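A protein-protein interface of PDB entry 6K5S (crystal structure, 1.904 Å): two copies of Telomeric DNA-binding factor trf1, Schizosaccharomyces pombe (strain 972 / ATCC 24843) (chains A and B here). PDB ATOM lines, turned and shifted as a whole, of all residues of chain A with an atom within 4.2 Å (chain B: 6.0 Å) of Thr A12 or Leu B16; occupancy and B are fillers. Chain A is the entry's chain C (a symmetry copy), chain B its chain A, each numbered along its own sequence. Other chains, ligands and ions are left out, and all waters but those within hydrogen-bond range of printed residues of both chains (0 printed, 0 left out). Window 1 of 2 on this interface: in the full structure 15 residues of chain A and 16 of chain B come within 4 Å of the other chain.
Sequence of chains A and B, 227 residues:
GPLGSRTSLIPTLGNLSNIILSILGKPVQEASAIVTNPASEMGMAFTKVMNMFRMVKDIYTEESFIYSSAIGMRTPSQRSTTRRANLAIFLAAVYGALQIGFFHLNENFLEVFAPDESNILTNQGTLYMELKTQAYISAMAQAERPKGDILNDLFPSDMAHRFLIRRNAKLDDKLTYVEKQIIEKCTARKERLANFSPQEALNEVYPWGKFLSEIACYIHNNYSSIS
The side-chain amide nitrogen (ND2) of Asn A15 sits at hydrogen-bond distance from the side-chain hydroxyl (OG1) of Thr B12, 2.6 Å away.
The side-chain amide nitrogen of Asn B15 sits at hydrogen-bond distance from the side-chain hydroxyl of Thr A12 (2.7 Å).
ND2 of Asn B15 touches CA of Leu A9 (3.6 Å).
Leu A9 touches Leu B16.
Ile B19 touches Leu A9 (CD1 to CD2, 3.6 Å).
Pro A11 touches Asn B15 (CG to OD1, 3.7 Å).
CG2 of Thr A12 touches OG1 of Thr B12, at 3.8 Å.
Thr A12 touches Leu B16.
Asn A15 touches Pro B11 (CG to CB, 3.7 Å).
Of chain B, only Thr B12, Asn B15 and Leu B16 come within 4 Å of Thr A12.
Of the printed residues of chain A, Ile B19 touches Leu A9.
Of the printed residues of chain A, Asn B15 touches Leu A9 (3.6 Å), Pro A11 (3.7 Å) and Thr A12 (2.7 Å).
Leu A16 touches none of the printed residues of chain B.
Phe B53 touches none of the printed residues of chain A.
The nearest printed residue of chain A that does not touch Thr B12 is Leu A16 (4.03 Å).
Hydrophobic or aromatic side chains of chain B within 4 Å of the printed part of chain A: Pro B11, Leu B16 and Ile B19.
Of the 8 printed residues of chain A, 4 touch a printed residue of chain B.
Hydrophobic or aromatic side chains of chain A within 4 Å of the printed part of chain B: Leu A9 and Pro A11.
Among the printed residues, no Asp or Glu carboxylate lies within 4 Å of a Lys or Arg side-chain nitrogen of the other chain.
Pro A11 touches Asn B15, and with the chains exchanged Asn A15 touches Pro B11.
Thr B12 touches its own counterpart, Thr A12.
Thr A12 touches Asn B15, and with the chains exchanged Asn A15 touches Thr B12.
Thr A12 touches Leu B16, but with the chains exchanged Leu A16 does not touch Thr B12 (4.03 Å).
6 positions are printed for both chains.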
ATOM      1  N   LEU A   9      -9.105  18.147  31.459  1.00  0.00           N
ATOM      2  CA  LEU A   9      -8.968  17.331  30.264  1.00  0.00           C
ATOM      3  C   LEU A   9     -10.219  17.344  29.389  1.00  0.00           C
ATOM      4  O   LEU A   9     -10.250  16.634  28.378  1.00  0.00           O
ATOM      5  CB  LEU A   9      -8.611  15.890  30.638  1.00  0.00           C
ATOM      6  CG  LEU A   9      -7.154  15.670  31.072  1.00  0.00           C
ATOM      7  CD1 LEU A   9      -6.959  14.336  31.782  1.00  0.00           C
ATOM      8  CD2 LEU A   9      -6.180  15.774  29.880  1.00  0.00           C
ATOM      9  N   ILE A  10     -11.225  18.150  29.728  1.00  0.00           N
ATOM     10  CA  ILE A  10     -12.482  18.219  28.972  1.00  0.00           C
ATOM     11  C   ILE A  10     -12.246  18.477  27.487  1.00  0.00           C
ATOM     12  O   ILE A  10     -12.883  17.814  26.663  1.00  0.00           O
ATOM     13  CB  ILE A  10     -13.442  19.268  29.562  1.00  0.00           C
ATOM     14  CG1 ILE A  10     -14.075  18.694  30.822  1.00  0.00           C
ATOM     15  CG2 ILE A  10     -14.558  19.613  28.535  1.00  0.00           C
ATOM     16  CD1 ILE A  10     -15.050  17.567  30.532  1.00  0.00           C
ATOM     17  N   PRO A  11     -11.364  19.399  27.078  1.00  0.00           N
ATOM     18  CA  PRO A  11     -11.135  19.559  25.632  1.00  0.00           C
ATOM     19  C   PRO A  11     -10.592  18.306  24.963  1.00  0.00           C
ATOM     20  O   PRO A  11     -10.932  18.044  23.808  1.00  0.00           O
ATOM     21  CB  PRO A  11     -10.132  20.721  25.552  1.00  0.00           C
ATOM     22  CG  PRO A  11     -10.280  21.447  26.846  1.00  0.00           C
ATOM     23  CD  PRO A  11     -10.581  20.384  27.857  1.00  0.00           C
ATOM     24  N   THR A  12      -9.753  17.523  25.637  1.00  0.00           N
ATOM     25  CA  THR A  12      -9.240  16.304  25.009  1.00  0.00           C
ATOM     26  C   THR A  12     -10.356  15.280  24.857  1.00  0.00           C
ATOM     27  O   THR A  12     -10.490  14.635  23.807  1.00  0.00           O
ATOM     28  CB  THR A  12      -8.075  15.712  25.837  1.00  0.00           C
ATOM     29  OG1 THR A  12      -6.910  16.533  25.722  1.00  0.00           O
ATOM     30  CG2 THR A  12      -7.706  14.312  25.341  1.00  0.00           C
ATOM     31  N   LEU A  13     -11.176  15.131  25.894  1.00  0.00           N
ATOM     32  CA  LEU A  13     -12.299  14.202  25.840  1.00  0.00           C
ATOM     33  C   LEU A  13     -13.251  14.548  24.689  1.00  0.00           C
ATOM     34  O   LEU A  13     -13.693  13.666  23.941  1.00  0.00           O
ATOM     35  CB  LEU A  13     -13.043  14.231  27.181  1.00  0.00           C
ATOM     36  CG  LEU A  13     -14.328  13.413  27.263  1.00  0.00           C
ATOM     37  CD1 LEU A  13     -13.943  11.983  27.054  1.00  0.00           C
ATOM     38  CD2 LEU A  13     -15.035  13.606  28.633  1.00  0.00           C
ATOM     39  N   GLY A  14     -13.595  15.831  24.554  1.00  0.00           N
ATOM     40  CA  GLY A  14     -14.493  16.232  23.486  1.00  0.00           C
ATOM     41  C   GLY A  14     -13.873  16.061  22.116  1.00  0.00           C
ATOM     42  O   GLY A  14     -14.558  15.696  21.157  1.00  0.00           O
ATOM     43  N   ASN A  15     -12.561  16.309  22.009  1.00  0.00           N
ATOM     44  CA  ASN A  15     -11.886  16.244  20.714  1.00  0.00           C
ATOM     45  C   ASN A  15     -11.813  14.810  20.215  1.00  0.00           C
ATOM     46  O   ASN A  15     -12.149  14.530  19.067  1.00  0.00           O
ATOM     47  CB  ASN A  15     -10.480  16.848  20.821  1.00  0.00           C
ATOM     48  CG  ASN A  15      -9.713  16.810  19.501  1.00  0.00           C
ATOM     49  OD1 ASN A  15     -10.237  17.163  18.430  1.00  0.00           O
ATOM     50  ND2 ASN A  15      -8.474  16.349  19.569  1.00  0.00           N
ATOM     51  N   LEU A  16     -11.351  13.897  21.067  1.00  0.00           N
ATOM     52  CA  LEU A  16     -11.332  12.477  20.727  1.00  0.00           C
ATOM     53  C   LEU A  16     -12.741  11.927  20.506  1.00  0.00           C
ATOM     54  O   LEU A  16     -12.949  11.112  19.598  1.00  0.00           O
ATOM     55  CB  LEU A  16     -10.623  11.683  21.822  1.00  0.00           C
ATOM     56  CG  LEU A  16      -9.153  12.002  22.021  1.00  0.00           C
ATOM     57  CD1 LEU A  16      -8.606  11.309  23.290  1.00  0.00           C
ATOM     58  CD2 LEU A  16      -8.365  11.607  20.754  1.00  0.00           C
ATOM     59  N   PRO B  11      -6.782  20.183  18.951  1.00  0.00           N
ATOM     60  CA  PRO B  11      -7.281  20.505  20.312  1.00  0.00           C
ATOM     61  C   PRO B  11      -6.681  19.641  21.420  1.00  0.00           C
ATOM     62  O   PRO B  11      -6.409  20.154  22.513  1.00  0.00           O
ATOM     63  CB  PRO B  11      -8.792  20.307  20.171  1.00  0.00           C
ATOM     64  CG  PRO B  11      -9.066  20.667  18.732  1.00  0.00           C
ATOM     65  CD  PRO B  11      -7.892  20.067  17.983  1.00  0.00           C
ATOM     66  N   THR B  12      -6.447  18.358  21.172  1.00  0.00           N
ATOM     67  CA  THR B  12      -5.822  17.494  22.177  1.00  0.00           C
ATOM     68  C   THR B  12      -4.358  17.876  22.394  1.00  0.00           C
ATOM     69  O   THR B  12      -3.902  18.032  23.536  1.00  0.00           O
ATOM     70  CB  THR B  12      -5.920  16.020  21.741  1.00  0.00           C
ATOM     71  OG1 THR B  12      -7.284  15.565  21.796  1.00  0.00           O
ATOM     72  CG2 THR B  12      -5.051  15.137  22.636  1.00  0.00           C
ATOM     73  N   LEU B  13      -3.598  18.009  21.297  1.00  0.00           N
ATOM     74  CA  LEU B  13      -2.229  18.486  21.384  1.00  0.00           C
ATOM     75  C   LEU B  13      -2.160  19.755  22.220  1.00  0.00           C
ATOM     76  O   LEU B  13      -1.341  19.860  23.129  1.00  0.00           O
ATOM     77  CB  LEU B  13      -1.656  18.741  19.978  1.00  0.00           C
ATOM     78  CG  LEU B  13      -0.166  19.123  19.984  1.00  0.00           C
ATOM     79  CD1 LEU B  13       0.677  17.996  20.574  1.00  0.00           C
ATOM     80  CD2 LEU B  13       0.327  19.433  18.560  1.00  0.00           C
ATOM     81  N   GLY B  14      -3.045  20.716  21.936  1.00  0.00           N
ATOM     82  CA  GLY B  14      -3.039  21.965  22.680  1.00  0.00           C
ATOM     83  C   GLY B  14      -3.408  21.798  24.144  1.00  0.00           C
ATOM     84  O   GLY B  14      -2.769  22.385  25.027  1.00  0.00           O
ATOM     85  N   ASN B  15      -4.446  21.003  24.429  1.00  0.00           N
ATOM     86  CA  ASN B  15      -4.891  20.842  25.811  1.00  0.00           C
ATOM     87  C   ASN B  15      -3.813  20.161  26.661  1.00  0.00           C
ATOM     88  O   ASN B  15      -3.472  20.621  27.760  1.00  0.00           O
ATOM     89  CB  ASN B  15      -6.185  20.035  25.811  1.00  0.00           C
ATOM     90  CG  ASN B  15      -6.769  19.838  27.191  1.00  0.00           C
ATOM     91  OD1 ASN B  15      -6.875  20.771  28.001  1.00  0.00           O
ATOM     92  ND2 ASN B  15      -7.224  18.633  27.442  1.00  0.00           N
ATOM     93  N   LEU B  16      -3.246  19.078  26.153  1.00  0.00           N
ATOM     94  CA  LEU B  16      -2.220  18.368  26.911  1.00  0.00           C
ATOM     95  C   LEU B  16      -0.980  19.226  27.081  1.00  0.00           C
ATOM     96  O   LEU B  16      -0.336  19.183  28.132  1.00  0.00           O
ATOM     97  CB  LEU B  16      -1.877  17.034  26.221  1.00  0.00           C
ATOM     98  CG  LEU B  16      -3.026  16.019  26.103  1.00  0.00           C
ATOM     99  CD1 LEU B  16      -2.611  14.794  25.245  1.00  0.00           C
ATOM    100  CD2 LEU B  16      -3.460  15.568  27.474  1.00  0.00           C
ATOM    101  N   SER B  17      -0.621  20.003  26.051  1.00  0.00           N
ATOM    102  CA  SER B  17       0.550  20.863  26.150  1.00  0.00           C
ATOM    103  C   SER B  17       0.339  21.911  27.223  1.00  0.00           C
ATOM    104  O   SER B  17       1.237  22.180  28.022  1.00  0.00           O
ATOM    105  CB  SER B  17       0.828  21.545  24.804  1.00  0.00           C
ATOM    106  OG  SER B  17       1.091  20.596  23.767  1.00  0.00           O
ATOM    107  N   ASN B  18      -0.854  22.503  27.247  1.00  0.00           N
ATOM    108  CA  ASN B  18      -1.185  23.515  28.248  1.00  0.00           C
ATOM    109  C   ASN B  18      -1.113  22.936  29.662  1.00  0.00           C
ATOM    110  O   ASN B  18      -0.574  23.568  30.576  1.00  0.00           O
ATOM    111  CB  ASN B  18      -2.578  24.081  27.961  1.00  0.00           C
ATOM    112  CG  ASN B  18      -2.629  24.987  26.698  1.00  0.00           C
ATOM    113  OD1 ASN B  18      -1.624  25.542  26.255  1.00  0.00           O
ATOM    114  ND2 ASN B  18      -3.827  25.173  26.165  1.00  0.00           N
ATOM    115  N   ILE B  19      -1.644  21.739  29.863  1.00  0.00           N
ATOM    116  CA  ILE B  19      -1.594  21.139  31.193  1.00  0.00           C
ATOM    117  C   ILE B  19      -0.142  20.912  31.618  1.00  0.00           C
ATOM    118  O   ILE B  19       0.255  21.224  32.747  1.00  0.00           O
ATOM    119  CB  ILE B  19      -2.415  19.839  31.219  1.00  0.00           C
ATOM    120  CG1 ILE B  19      -3.909  20.163  31.046  1.00  0.00           C
ATOM    121  CG2 ILE B  19      -2.141  19.058  32.483  1.00  0.00           C
ATOM    122  CD1 ILE B  19      -4.787  18.931  30.749  1.00  0.00           C
ATOM    123  N   ILE B  20       0.676  20.374  30.709  1.00  0.00           N
ATOM    124  CA  ILE B  20       2.073  20.118  31.040  1.00  0.00           C
ATOM    125  C   ILE B  20       2.794  21.425  31.374  1.00  0.00           C
ATOM    126  O   ILE B  20       3.546  21.512  32.356  1.00  0.00           O
ATOM    127  CB  ILE B  20       2.746  19.361  29.875  1.00  0.00           C
ATOM    128  CG1 ILE B  20       2.104  17.991  29.725  1.00  0.00           C
ATOM    129  CG2 ILE B  20       4.273  19.288  30.061  1.00  0.00           C
ATOM    130  CD1 ILE B  20       2.447  17.321  28.418  1.00  0.00           C
ATOM    131  N   LEU B  21       2.565  22.468  30.573  1.00  0.00           N
ATOM    132  CA  LEU B  21       3.244  23.734  30.817  1.00  0.00           C
ATOM    133  C   LEU B  21       2.860  24.315  32.171  1.00  0.00           C
ATOM    134  O   LEU B  21       3.708  24.861  32.886  1.00  0.00           O
ATOM    135  CB  LEU B  21       2.916  24.733  29.718  1.00  0.00           C
ATOM    136  CG  LEU B  21       3.684  24.377  28.453  1.00  0.00           C
ATOM    137  CD1 LEU B  21       3.045  25.107  27.256  1.00  0.00           C
ATOM    138  CD2 LEU B  21       5.144  24.717  28.638  1.00  0.00           C
ATOM    139  N   VAL B  49      -1.414  12.243  32.119  1.00  0.00           N
ATOM    140  CA  VAL B  49      -1.277  13.308  31.123  1.00  0.00           C
ATOM    141  C   VAL B  49      -0.049  13.067  30.250  1.00  0.00           C
ATOM    142  O   VAL B  49      -0.115  13.174  29.017  1.00  0.00           O
ATOM    143  CB  VAL B  49      -1.221  14.681  31.814  1.00  0.00           C
ATOM    144  CG1 VAL B  49      -0.785  15.750  30.836  1.00  0.00           C
ATOM    145  CG2 VAL B  49      -2.605  15.009  32.391  1.00  0.00           C
ATOM    146  N   MET B  52      -0.633  10.248  27.731  1.00  0.00           N
ATOM    147  CA  MET B  52      -1.416  10.683  26.579  1.00  0.00           C
ATOM    148  C   MET B  52      -0.583  11.605  25.699  1.00  0.00           C
ATOM    149  O   MET B  52      -0.657  11.521  24.467  1.00  0.00           O
ATOM    150  CB  MET B  52      -2.715  11.368  27.021  1.00  0.00           C
ATOM    151  CG  MET B  52      -3.876  10.379  27.416  1.00  0.00           C
ATOM    152  SD  MET B  52      -5.359  11.236  28.062  1.00  0.00           S
ATOM    153  CE  MET B  52      -4.618  12.033  29.445  1.00  0.00           C
ATOM    154  N   PHE B  53       0.240  12.456  26.313  1.00  0.00           N
ATOM    155  CA  PHE B  53       1.033  13.401  25.535  1.00  0.00           C
ATOM    156  C   PHE B  53       2.038  12.666  24.656  1.00  0.00           C
ATOM    157  O   PHE B  53       2.165  12.957  23.466  1.00  0.00           O
ATOM    158  CB  PHE B  53       1.741  14.397  26.444  1.00  0.00           C
ATOM    159  CG  PHE B  53       2.445  15.507  25.696  1.00  0.00           C
ATOM    160  CD1 PHE B  53       1.715  16.440  24.965  1.00  0.00           C
ATOM    161  CD2 PHE B  53       3.824  15.613  25.716  1.00  0.00           C
ATOM    162  CE1 PHE B  53       2.360  17.466  24.282  1.00  0.00           C
ATOM    163  CE2 PHE B  53       4.472  16.617  25.030  1.00  0.00           C
ATOM    164  CZ  PHE B  53       3.731  17.553  24.309  1.00  0.00           C
ATOM    165  N   VAL B  56       0.147  11.384  21.633  1.00  0.00           N
ATOM    166  CA  VAL B  56      -0.239  12.399  20.651  1.00  0.00           C
ATOM    167  C   VAL B  56       1.001  12.968  19.968  1.00  0.00           C
ATOM    168  O   VAL B  56       0.990  13.207  18.758  1.00  0.00           O
ATOM    169  CB  VAL B  56      -1.109  13.499  21.291  1.00  0.00           C
ATOM    170  CG1 VAL B  56      -0.329  14.362  22.206  1.00  0.00           C
ATOM    171  CG2 VAL B  56      -1.748  14.392  20.207  1.00  0.00           C
ATOM    172  N   ALA B  88       6.166  22.722  25.725  1.00  0.00           N
ATOM    173  CA  ALA B  88       5.855  21.683  26.700  1.00  0.00           C
ATOM    174  C   ALA B  88       6.856  20.545  26.597  1.00  0.00           C
ATOM    175  O   ALA B  88       7.306  20.007  27.620  1.00  0.00           O
ATOM    176  CB  ALA B  88       4.422  21.181  26.501  1.00  0.00           C
